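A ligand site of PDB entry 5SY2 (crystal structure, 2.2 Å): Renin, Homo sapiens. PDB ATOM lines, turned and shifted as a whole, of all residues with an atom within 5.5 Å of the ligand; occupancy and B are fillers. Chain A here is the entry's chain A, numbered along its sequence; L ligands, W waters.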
ATOM      1  N   THR A  18     -15.097  21.401 -13.066  1.00  0.00           N
ATOM      2  CA  THR A  18     -14.586  22.661 -13.639  1.00  0.00           C
ATOM      3  C   THR A  18     -14.041  22.515 -15.061  1.00  0.00           C
ATOM      4  O   THR A  18     -13.997  23.511 -15.796  1.00  0.00           O
ATOM      5  CB  THR A  18     -13.503  23.302 -12.761  1.00  0.00           C
ATOM      6  OG1 THR A  18     -12.377  22.431 -12.672  1.00  0.00           O
ATOM      7  CG2 THR A  18     -14.005  23.601 -11.365  1.00  0.00           C
ATOM      8  N   GLN A  19     -13.615  21.318 -15.447  1.00  0.00           N
ATOM      9  CA  GLN A  19     -13.037  21.077 -16.752  1.00  0.00           C
ATOM     10  C   GLN A  19     -13.630  19.815 -17.365  1.00  0.00           C
ATOM     11  O   GLN A  19     -13.572  18.757 -16.764  1.00  0.00           O
ATOM     12  CB  GLN A  19     -11.519  20.953 -16.628  1.00  0.00           C
ATOM     13  CG  GLN A  19     -10.829  22.143 -15.964  1.00  0.00           C
ATOM     14  CD  GLN A  19      -9.323  21.996 -15.874  1.00  0.00           C
ATOM     15  OE1 GLN A  19      -8.709  21.271 -16.635  1.00  0.00           O
ATOM     16  NE2 GLN A  19      -8.718  22.705 -14.935  1.00  0.00           N
ATOM     17  N   TYR A  20     -14.237  19.971 -18.530  1.00  0.00           N
ATOM     18  CA  TYR A  20     -14.791  18.895 -19.341  1.00  0.00           C
ATOM     19  C   TYR A  20     -14.009  18.857 -20.647  1.00  0.00           C
ATOM     20  O   TYR A  20     -13.850  19.870 -21.321  1.00  0.00           O
ATOM     21  CB  TYR A  20     -16.285  19.125 -19.621  1.00  0.00           C
ATOM     22  CG  TYR A  20     -17.128  19.065 -18.370  1.00  0.00           C
ATOM     23  CD1 TYR A  20     -17.226  20.178 -17.529  1.00  0.00           C
ATOM     24  CD2 TYR A  20     -17.810  17.915 -18.027  1.00  0.00           C
ATOM     25  CE1 TYR A  20     -17.987  20.131 -16.375  1.00  0.00           C
ATOM     26  CE2 TYR A  20     -18.592  17.864 -16.880  1.00  0.00           C
ATOM     27  CZ  TYR A  20     -18.682  18.980 -16.062  1.00  0.00           C
ATOM     28  OH  TYR A  20     -19.434  18.952 -14.915  1.00  0.00           O
ATOM     29  N   VAL A  36     -10.765  20.727 -24.661  1.00  0.00           N
ATOM     30  CA  VAL A  36     -12.061  21.314 -24.327  1.00  0.00           C
ATOM     31  C   VAL A  36     -12.773  21.641 -25.621  1.00  0.00           C
ATOM     32  O   VAL A  36     -12.189  22.287 -26.500  1.00  0.00           O
ATOM     33  CB  VAL A  36     -11.895  22.612 -23.517  1.00  0.00           C
ATOM     34  CG1 VAL A  36     -13.226  23.324 -23.332  1.00  0.00           C
ATOM     35  CG2 VAL A  36     -11.269  22.321 -22.166  1.00  0.00           C
ATOM     36  N   ASP A  38     -15.306  24.013 -27.093  1.00  0.00           N
ATOM     37  CA  ASP A  38     -15.545  25.355 -26.570  1.00  0.00           C
ATOM     38  C   ASP A  38     -16.397  26.191 -27.516  1.00  0.00           C
ATOM     39  O   ASP A  38     -15.897  26.705 -28.512  1.00  0.00           O
ATOM     40  CB  ASP A  38     -14.174  26.019 -26.358  1.00  0.00           C
ATOM     41  CG  ASP A  38     -14.258  27.463 -25.872  1.00  0.00           C
ATOM     42  OD1 ASP A  38     -15.277  27.862 -25.276  1.00  0.00           O
ATOM     43  OD2 ASP A  38     -13.285  28.223 -26.105  1.00  0.00           O
ATOM     44  N   GLY A  40     -17.408  29.138 -26.901  1.00  0.00           N
ATOM     45  CA  GLY A  40     -16.966  30.522 -26.759  1.00  0.00           C
ATOM     46  C   GLY A  40     -15.781  30.968 -27.607  1.00  0.00           C
ATOM     47  O   GLY A  40     -15.378  32.121 -27.538  1.00  0.00           O
ATOM     48  N   SER A  41     -15.205  30.070 -28.398  1.00  0.00           N
ATOM     49  CA  SER A  41     -14.133  30.397 -29.323  1.00  0.00           C
ATOM     50  C   SER A  41     -14.255  29.519 -30.575  1.00  0.00           C
ATOM     51  O   SER A  41     -14.948  28.497 -30.586  1.00  0.00           O
ATOM     52  CB  SER A  41     -12.781  30.175 -28.674  1.00  0.00           C
ATOM     53  OG  SER A  41     -12.515  28.788 -28.490  1.00  0.00           O
ATOM     54  N   TYR A  83      -7.958  34.974 -24.871  1.00  0.00           N
ATOM     55  CA  TYR A  83      -9.119  34.645 -24.056  1.00  0.00           C
ATOM     56  C   TYR A  83      -9.222  35.573 -22.839  1.00  0.00           C
ATOM     57  O   TYR A  83      -8.260  36.237 -22.472  1.00  0.00           O
ATOM     58  CB  TYR A  83      -9.027  33.206 -23.544  1.00  0.00           C
ATOM     59  CG  TYR A  83      -8.899  32.140 -24.617  1.00  0.00           C
ATOM     60  CD1 TYR A  83      -9.831  32.045 -25.659  1.00  0.00           C
ATOM     61  CD2 TYR A  83      -7.874  31.195 -24.570  1.00  0.00           C
ATOM     62  CE1 TYR A  83      -9.726  31.060 -26.622  1.00  0.00           C
ATOM     63  CE2 TYR A  83      -7.760  30.197 -25.538  1.00  0.00           C
ATOM     64  CZ  TYR A  83      -8.691  30.131 -26.559  1.00  0.00           C
ATOM     65  OH  TYR A  83      -8.596  29.149 -27.511  1.00  0.00           O
ATOM     66  N   SER A  84     -10.387  35.569 -22.216  1.00  0.00           N
ATOM     67  CA  SER A  84     -10.604  36.329 -20.973  1.00  0.00           C
ATOM     68  C   SER A  84      -9.802  35.778 -19.785  1.00  0.00           C
ATOM     69  O   SER A  84      -9.547  36.499 -18.816  1.00  0.00           O
ATOM     70  CB  SER A  84     -12.103  36.366 -20.630  1.00  0.00           C
ATOM     71  OG  SER A  84     -12.666  35.051 -20.619  1.00  0.00           O
ATOM     72  N   THR A  85      -9.390  34.507 -19.866  1.00  0.00           N
ATOM     73  CA  THR A  85      -8.645  33.834 -18.801  1.00  0.00           C
ATOM     74  C   THR A  85      -7.136  33.737 -19.049  1.00  0.00           C
ATOM     75  O   THR A  85      -6.403  33.243 -18.196  1.00  0.00           O
ATOM     76  CB  THR A  85      -9.199  32.410 -18.591  1.00  0.00           C
ATOM     77  OG1 THR A  85      -9.381  31.783 -19.876  1.00  0.00           O
ATOM     78  CG2 THR A  85     -10.540  32.482 -17.877  1.00  0.00           C
ATOM     79  N   PRO A 118      -3.060  30.392 -16.947  1.00  0.00           N
ATOM     80  CA  PRO A 118      -3.723  29.324 -16.198  1.00  0.00           C
ATOM     81  C   PRO A 118      -3.370  27.874 -16.595  1.00  0.00           C
ATOM     82  O   PRO A 118      -3.908  26.939 -15.998  1.00  0.00           O
ATOM     83  CB  PRO A 118      -5.193  29.571 -16.550  1.00  0.00           C
ATOM     84  CG  PRO A 118      -5.127  30.012 -17.981  1.00  0.00           C
ATOM     85  CD  PRO A 118      -3.817  30.748 -18.154  1.00  0.00           C
ATOM     86  N   PHE A 119      -2.489  27.678 -17.585  1.00  0.00           N
ATOM     87  CA  PHE A 119      -2.381  26.367 -18.238  1.00  0.00           C
ATOM     88  C   PHE A 119      -1.702  25.263 -17.417  1.00  0.00           C
ATOM     89  O   PHE A 119      -1.949  24.095 -17.672  1.00  0.00           O
ATOM     90  CB  PHE A 119      -1.833  26.499 -19.654  1.00  0.00           C
ATOM     91  CG  PHE A 119      -2.749  27.275 -20.553  1.00  0.00           C
ATOM     92  CD1 PHE A 119      -3.933  26.687 -21.028  1.00  0.00           C
ATOM     93  CD2 PHE A 119      -2.482  28.612 -20.872  1.00  0.00           C
ATOM     94  CE1 PHE A 119      -4.800  27.424 -21.832  1.00  0.00           C
ATOM     95  CE2 PHE A 119      -3.348  29.340 -21.672  1.00  0.00           C
ATOM     96  CZ  PHE A 119      -4.512  28.753 -22.149  1.00  0.00           C
ATOM     97  N   LEU A 121      -2.755  24.795 -14.504  1.00  0.00           N
ATOM     98  CA  LEU A 121      -3.963  24.294 -13.837  1.00  0.00           C
ATOM     99  C   LEU A 121      -4.914  23.498 -14.754  1.00  0.00           C
ATOM    100  O   LEU A 121      -5.937  23.024 -14.280  1.00  0.00           O
ATOM    101  CB  LEU A 121      -4.729  25.445 -13.199  1.00  0.00           C
ATOM    102  CG  LEU A 121      -3.964  26.409 -12.288  1.00  0.00           C
ATOM    103  CD1 LEU A 121      -4.913  27.513 -11.812  1.00  0.00           C
ATOM    104  CD2 LEU A 121      -3.358  25.703 -11.084  1.00  0.00           C
ATOM    105  N   ALA A 122      -4.588  23.348 -16.032  1.00  0.00           N
ATOM    106  CA  ALA A 122      -5.445  22.649 -16.990  1.00  0.00           C
ATOM    107  C   ALA A 122      -5.108  21.167 -17.086  1.00  0.00           C
ATOM    108  O   ALA A 122      -3.937  20.811 -17.260  1.00  0.00           O
ATOM    109  CB  ALA A 122      -5.321  23.279 -18.375  1.00  0.00           C
ATOM    110  N   PHE A 124      -6.661  19.493 -19.477  1.00  0.00           N
ATOM    111  CA  PHE A 124      -6.691  19.436 -20.913  1.00  0.00           C
ATOM    112  C   PHE A 124      -5.400  19.998 -21.512  1.00  0.00           C
ATOM    113  O   PHE A 124      -4.722  20.801 -20.889  1.00  0.00           O
ATOM    114  CB  PHE A 124      -7.919  20.175 -21.448  1.00  0.00           C
ATOM    115  CG  PHE A 124      -7.984  21.652 -21.081  1.00  0.00           C
ATOM    116  CD1 PHE A 124      -8.649  22.064 -19.938  1.00  0.00           C
ATOM    117  CD2 PHE A 124      -7.434  22.610 -21.911  1.00  0.00           C
ATOM    118  CE1 PHE A 124      -8.733  23.419 -19.612  1.00  0.00           C
ATOM    119  CE2 PHE A 124      -7.509  23.953 -21.591  1.00  0.00           C
ATOM    120  CZ  PHE A 124      -8.163  24.359 -20.436  1.00  0.00           C
ATOM    121  N   VAL A 127      -7.712  23.151 -27.061  1.00  0.00           N
ATOM    122  CA  VAL A 127      -9.103  23.572 -27.236  1.00  0.00           C
ATOM    123  C   VAL A 127      -9.556  23.266 -28.650  1.00  0.00           C
ATOM    124  O   VAL A 127      -8.802  23.462 -29.592  1.00  0.00           O
ATOM    125  CB  VAL A 127      -9.240  25.105 -27.001  1.00  0.00           C
ATOM    126  CG1 VAL A 127     -10.678  25.571 -27.253  1.00  0.00           C
ATOM    127  CG2 VAL A 127      -8.799  25.461 -25.594  1.00  0.00           C
ATOM    128  N   TYR A 162     -23.047  17.604 -19.788  1.00  0.00           N
ATOM    129  CA  TYR A 162     -22.032  17.646 -18.731  1.00  0.00           C
ATOM    130  C   TYR A 162     -22.638  17.027 -17.477  1.00  0.00           C
ATOM    131  O   TYR A 162     -23.614  17.549 -16.928  1.00  0.00           O
ATOM    132  CB  TYR A 162     -21.579  19.087 -18.429  1.00  0.00           C
ATOM    133  CG  TYR A 162     -20.633  19.741 -19.432  1.00  0.00           C
ATOM    134  CD1 TYR A 162     -20.000  19.030 -20.454  1.00  0.00           C
ATOM    135  CD2 TYR A 162     -20.334  21.091 -19.331  1.00  0.00           C
ATOM    136  CE1 TYR A 162     -19.144  19.645 -21.340  1.00  0.00           C
ATOM    137  CE2 TYR A 162     -19.478  21.715 -20.221  1.00  0.00           C
ATOM    138  CZ  TYR A 162     -18.873  20.988 -21.225  1.00  0.00           C
ATOM    139  OH  TYR A 162     -18.015  21.588 -22.095  1.00  0.00           O
ATOM    140  N   ASP A 226     -21.328  29.288 -23.197  1.00  0.00           N
ATOM    141  CA  ASP A 226     -19.916  28.961 -23.356  1.00  0.00           C
ATOM    142  C   ASP A 226     -19.515  27.617 -22.718  1.00  0.00           C
ATOM    143  O   ASP A 226     -19.120  27.537 -21.544  1.00  0.00           O
ATOM    144  CB  ASP A 226     -19.051  30.098 -22.780  1.00  0.00           C
ATOM    145  CG  ASP A 226     -17.565  29.926 -23.085  1.00  0.00           C
ATOM    146  OD1 ASP A 226     -17.167  28.876 -23.649  1.00  0.00           O
ATOM    147  OD2 ASP A 226     -16.783  30.831 -22.761  1.00  0.00           O
ATOM    148  N   THR A 227     -19.559  26.576 -23.543  1.00  0.00           N
ATOM    149  CA  THR A 227     -19.253  25.225 -23.088  1.00  0.00           C
ATOM    150  C   THR A 227     -17.841  25.091 -22.528  1.00  0.00           C
ATOM    151  O   THR A 227     -17.582  24.185 -21.739  1.00  0.00           O
ATOM    152  CB  THR A 227     -19.432  24.183 -24.223  1.00  0.00           C
ATOM    153  OG1 THR A 227     -18.584  24.509 -25.324  1.00  0.00           O
ATOM    154  CG2 THR A 227     -20.872  24.147 -24.688  1.00  0.00           C
ATOM    155  N   GLY A 228     -16.927  25.980 -22.952  1.00  0.00           N
ATOM    156  CA  GLY A 228     -15.555  25.960 -22.484  1.00  0.00           C
ATOM    157  C   GLY A 228     -15.262  26.658 -21.168  1.00  0.00           C
ATOM    158  O   GLY A 228     -14.112  26.631 -20.714  1.00  0.00           O
ATOM    159  N   ALA A 229     -16.267  27.295 -20.563  1.00  0.00           N
ATOM    160  CA  ALA A 229     -16.087  27.983 -19.289  1.00  0.00           C
ATOM    161  C   ALA A 229     -16.624  27.130 -18.136  1.00  0.00           C
ATOM    162  O   ALA A 229     -17.669  26.484 -18.259  1.00  0.00           O
ATOM    163  CB  ALA A 229     -16.771  29.350 -19.310  1.00  0.00           C
ATOM    164  N   SER A 230     -15.915  27.169 -17.005  1.00  0.00           N
ATOM    165  CA  SER A 230     -16.292  26.401 -15.819  1.00  0.00           C
ATOM    166  C   SER A 230     -17.571  26.941 -15.171  1.00  0.00           C
ATOM    167  O   SER A 230     -18.415  26.178 -14.701  1.00  0.00           O
ATOM    168  CB  SER A 230     -15.158  26.420 -14.784  1.00  0.00           C
ATOM    169  OG  SER A 230     -13.890  26.137 -15.364  1.00  0.00           O
ATOM    170  N   ALA A 317     -20.262  25.706 -17.580  1.00  0.00           N
ATOM    171  CA  ALA A 317     -20.590  24.341 -17.151  1.00  0.00           C
ATOM    172  C   ALA A 317     -21.580  24.265 -15.981  1.00  0.00           C
ATOM    173  O   ALA A 317     -22.372  23.343 -15.936  1.00  0.00           O
ATOM    174  CB  ALA A 317     -19.327  23.564 -16.818  1.00  0.00           C
HETATM  175  N1  LIG L   1     -11.334  28.911 -21.415  1.00  0.00           N
HETATM  176  C1  LIG L   1     -12.373  29.754 -22.074  1.00  0.00           C
HETATM  177  C2  LIG L   1     -11.788  30.952 -22.865  1.00  0.00           C
HETATM  178  C3  LIG L   1     -12.866  31.861 -23.482  1.00  0.00           C
HETATM  179  C4  LIG L   1     -13.813  31.015 -24.359  1.00  0.00           C
HETATM  180  C5  LIG L   1     -11.474  28.771 -20.055  1.00  0.00           C
HETATM  181  C6  LIG L   1      -9.369  28.633 -18.721  1.00  0.00           C
HETATM  182  C7  LIG L   1      -8.825  26.772 -17.469  1.00  0.00           C
HETATM  183  C8  LIG L   1     -12.386  24.808 -18.321  1.00  0.00           C
HETATM  184  C9  LIG L   1     -13.611  24.196 -18.944  1.00  0.00           C
HETATM  185  C10 LIG L   1     -13.632  23.302 -19.931  1.00  0.00           C
HETATM  186  C11 LIG L   1     -15.716  23.756 -19.336  1.00  0.00           C
HETATM  187  C12 LIG L   1     -10.506  26.831 -22.521  1.00  0.00           C
HETATM  188  C13 LIG L   1     -10.220  28.303 -22.166  1.00  0.00           C
HETATM  189  N2  LIG L   1     -14.361  29.879 -23.582  1.00  0.00           N
HETATM  190  C14 LIG L   1     -13.353  28.977 -22.964  1.00  0.00           C
HETATM  191  O1  LIG L   1     -12.420  29.307 -19.503  1.00  0.00           O
HETATM  192  C15 LIG L   1     -10.559  28.014 -19.163  1.00  0.00           C
HETATM  193  N3  LIG L   1      -8.544  27.993 -17.907  1.00  0.00           N
HETATM  194  C16 LIG L   1      -7.850  26.094 -16.545  1.00  0.00           C
HETATM  195  N4  LIG L   1      -9.929  26.141 -17.838  1.00  0.00           N
HETATM  196  C17 LIG L   1     -10.834  26.706 -18.673  1.00  0.00           C
HETATM  197  N5  LIG L   1     -11.976  26.020 -19.041  1.00  0.00           N
HETATM  198  C18 LIG L   1     -14.989  23.023 -20.197  1.00  0.00           C
HETATM  199  O2  LIG L   1     -14.875  24.466 -18.583  1.00  0.00           O
HETATM  200  O   HOH W   1     -13.595  29.043 -16.922  1.00  0.00           O
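The side-chain carboxylate (OD2) of Asp 226 lies within salt-bridge range of a nitrogen (N2) of the ligand (2.7 Å).
N5 of the ligand lies within hydrogen-bond range of O of Gly 228.
The side-chain carboxylate (OD1) of Asp 38 lies within salt-bridge range of a nitrogen (N2) of the ligand (2.8 Å).
The backbone NH (N) of Ser 230 lies within hydrogen-bond range of an oxygen (O2) of the ligand (3.3 Å).
The side-chain carboxylate of Asp 226 is in hydrogen-bond range of the backbone NH of Gly 228, at 3.0 Å.
The side-chain carboxylate (OD1) of Asp 226 sits close to the side-chain carboxylate (OD1) of Asp 38 (2.7 Å).
N of Gly 40 lies within hydrogen-bond range of OD1 of Asp 226.
The side-chain carboxylate (OD1) of Asp 38 sits close to the backbone NH (N) of Gly 228, at 3.4 Å.
The backbone carbonyl oxygen (O) of Thr 227 lies within hydrogen-bond range of the side-chain hydroxyl (OH) of Tyr 162 (2.7 Å).
The side-chain hydroxyl (OG) of Ser 230 sits at hydrogen-bond distance from the backbone carbonyl oxygen (O) of Thr 18.
The backbone carbonyl oxygen of Ser 230 sits at hydrogen-bond distance from the backbone NH of Ala 317 (3.5 Å).
The side-chain amide nitrogen (NE2) of Gln 19 lies within hydrogen-bond range of the backbone carbonyl oxygen (O) of Leu 121 (2.9 Å).
The backbone carbonyl oxygen (O) of Thr 18 sits close to an oxygen (O2) of the ligand, at 3.1 Å.
O of Ala 229 sits close to O2 of the ligand, at 3.5 Å.
Residues that only touch the ligand: Gln 19, Tyr 20, Val 36, Gly 40, Tyr 83, Thr 85, Pro 118, Phe 124, Val 127, Tyr 162 and Thr 227.
Hydrophobic or aromatic side chains that line the ligand: Val 36, Tyr 83, Pro 118, Phe 124 and Val 127.
The nearest printed residue that does not touch the ligand is Ala 122 (4.2 Å).
Water W1 lies within hydrogen-bond range of an oxygen (O1) of the ligand (2.8 Å) and the backbone NH of Ser 230 (3.0 Å).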
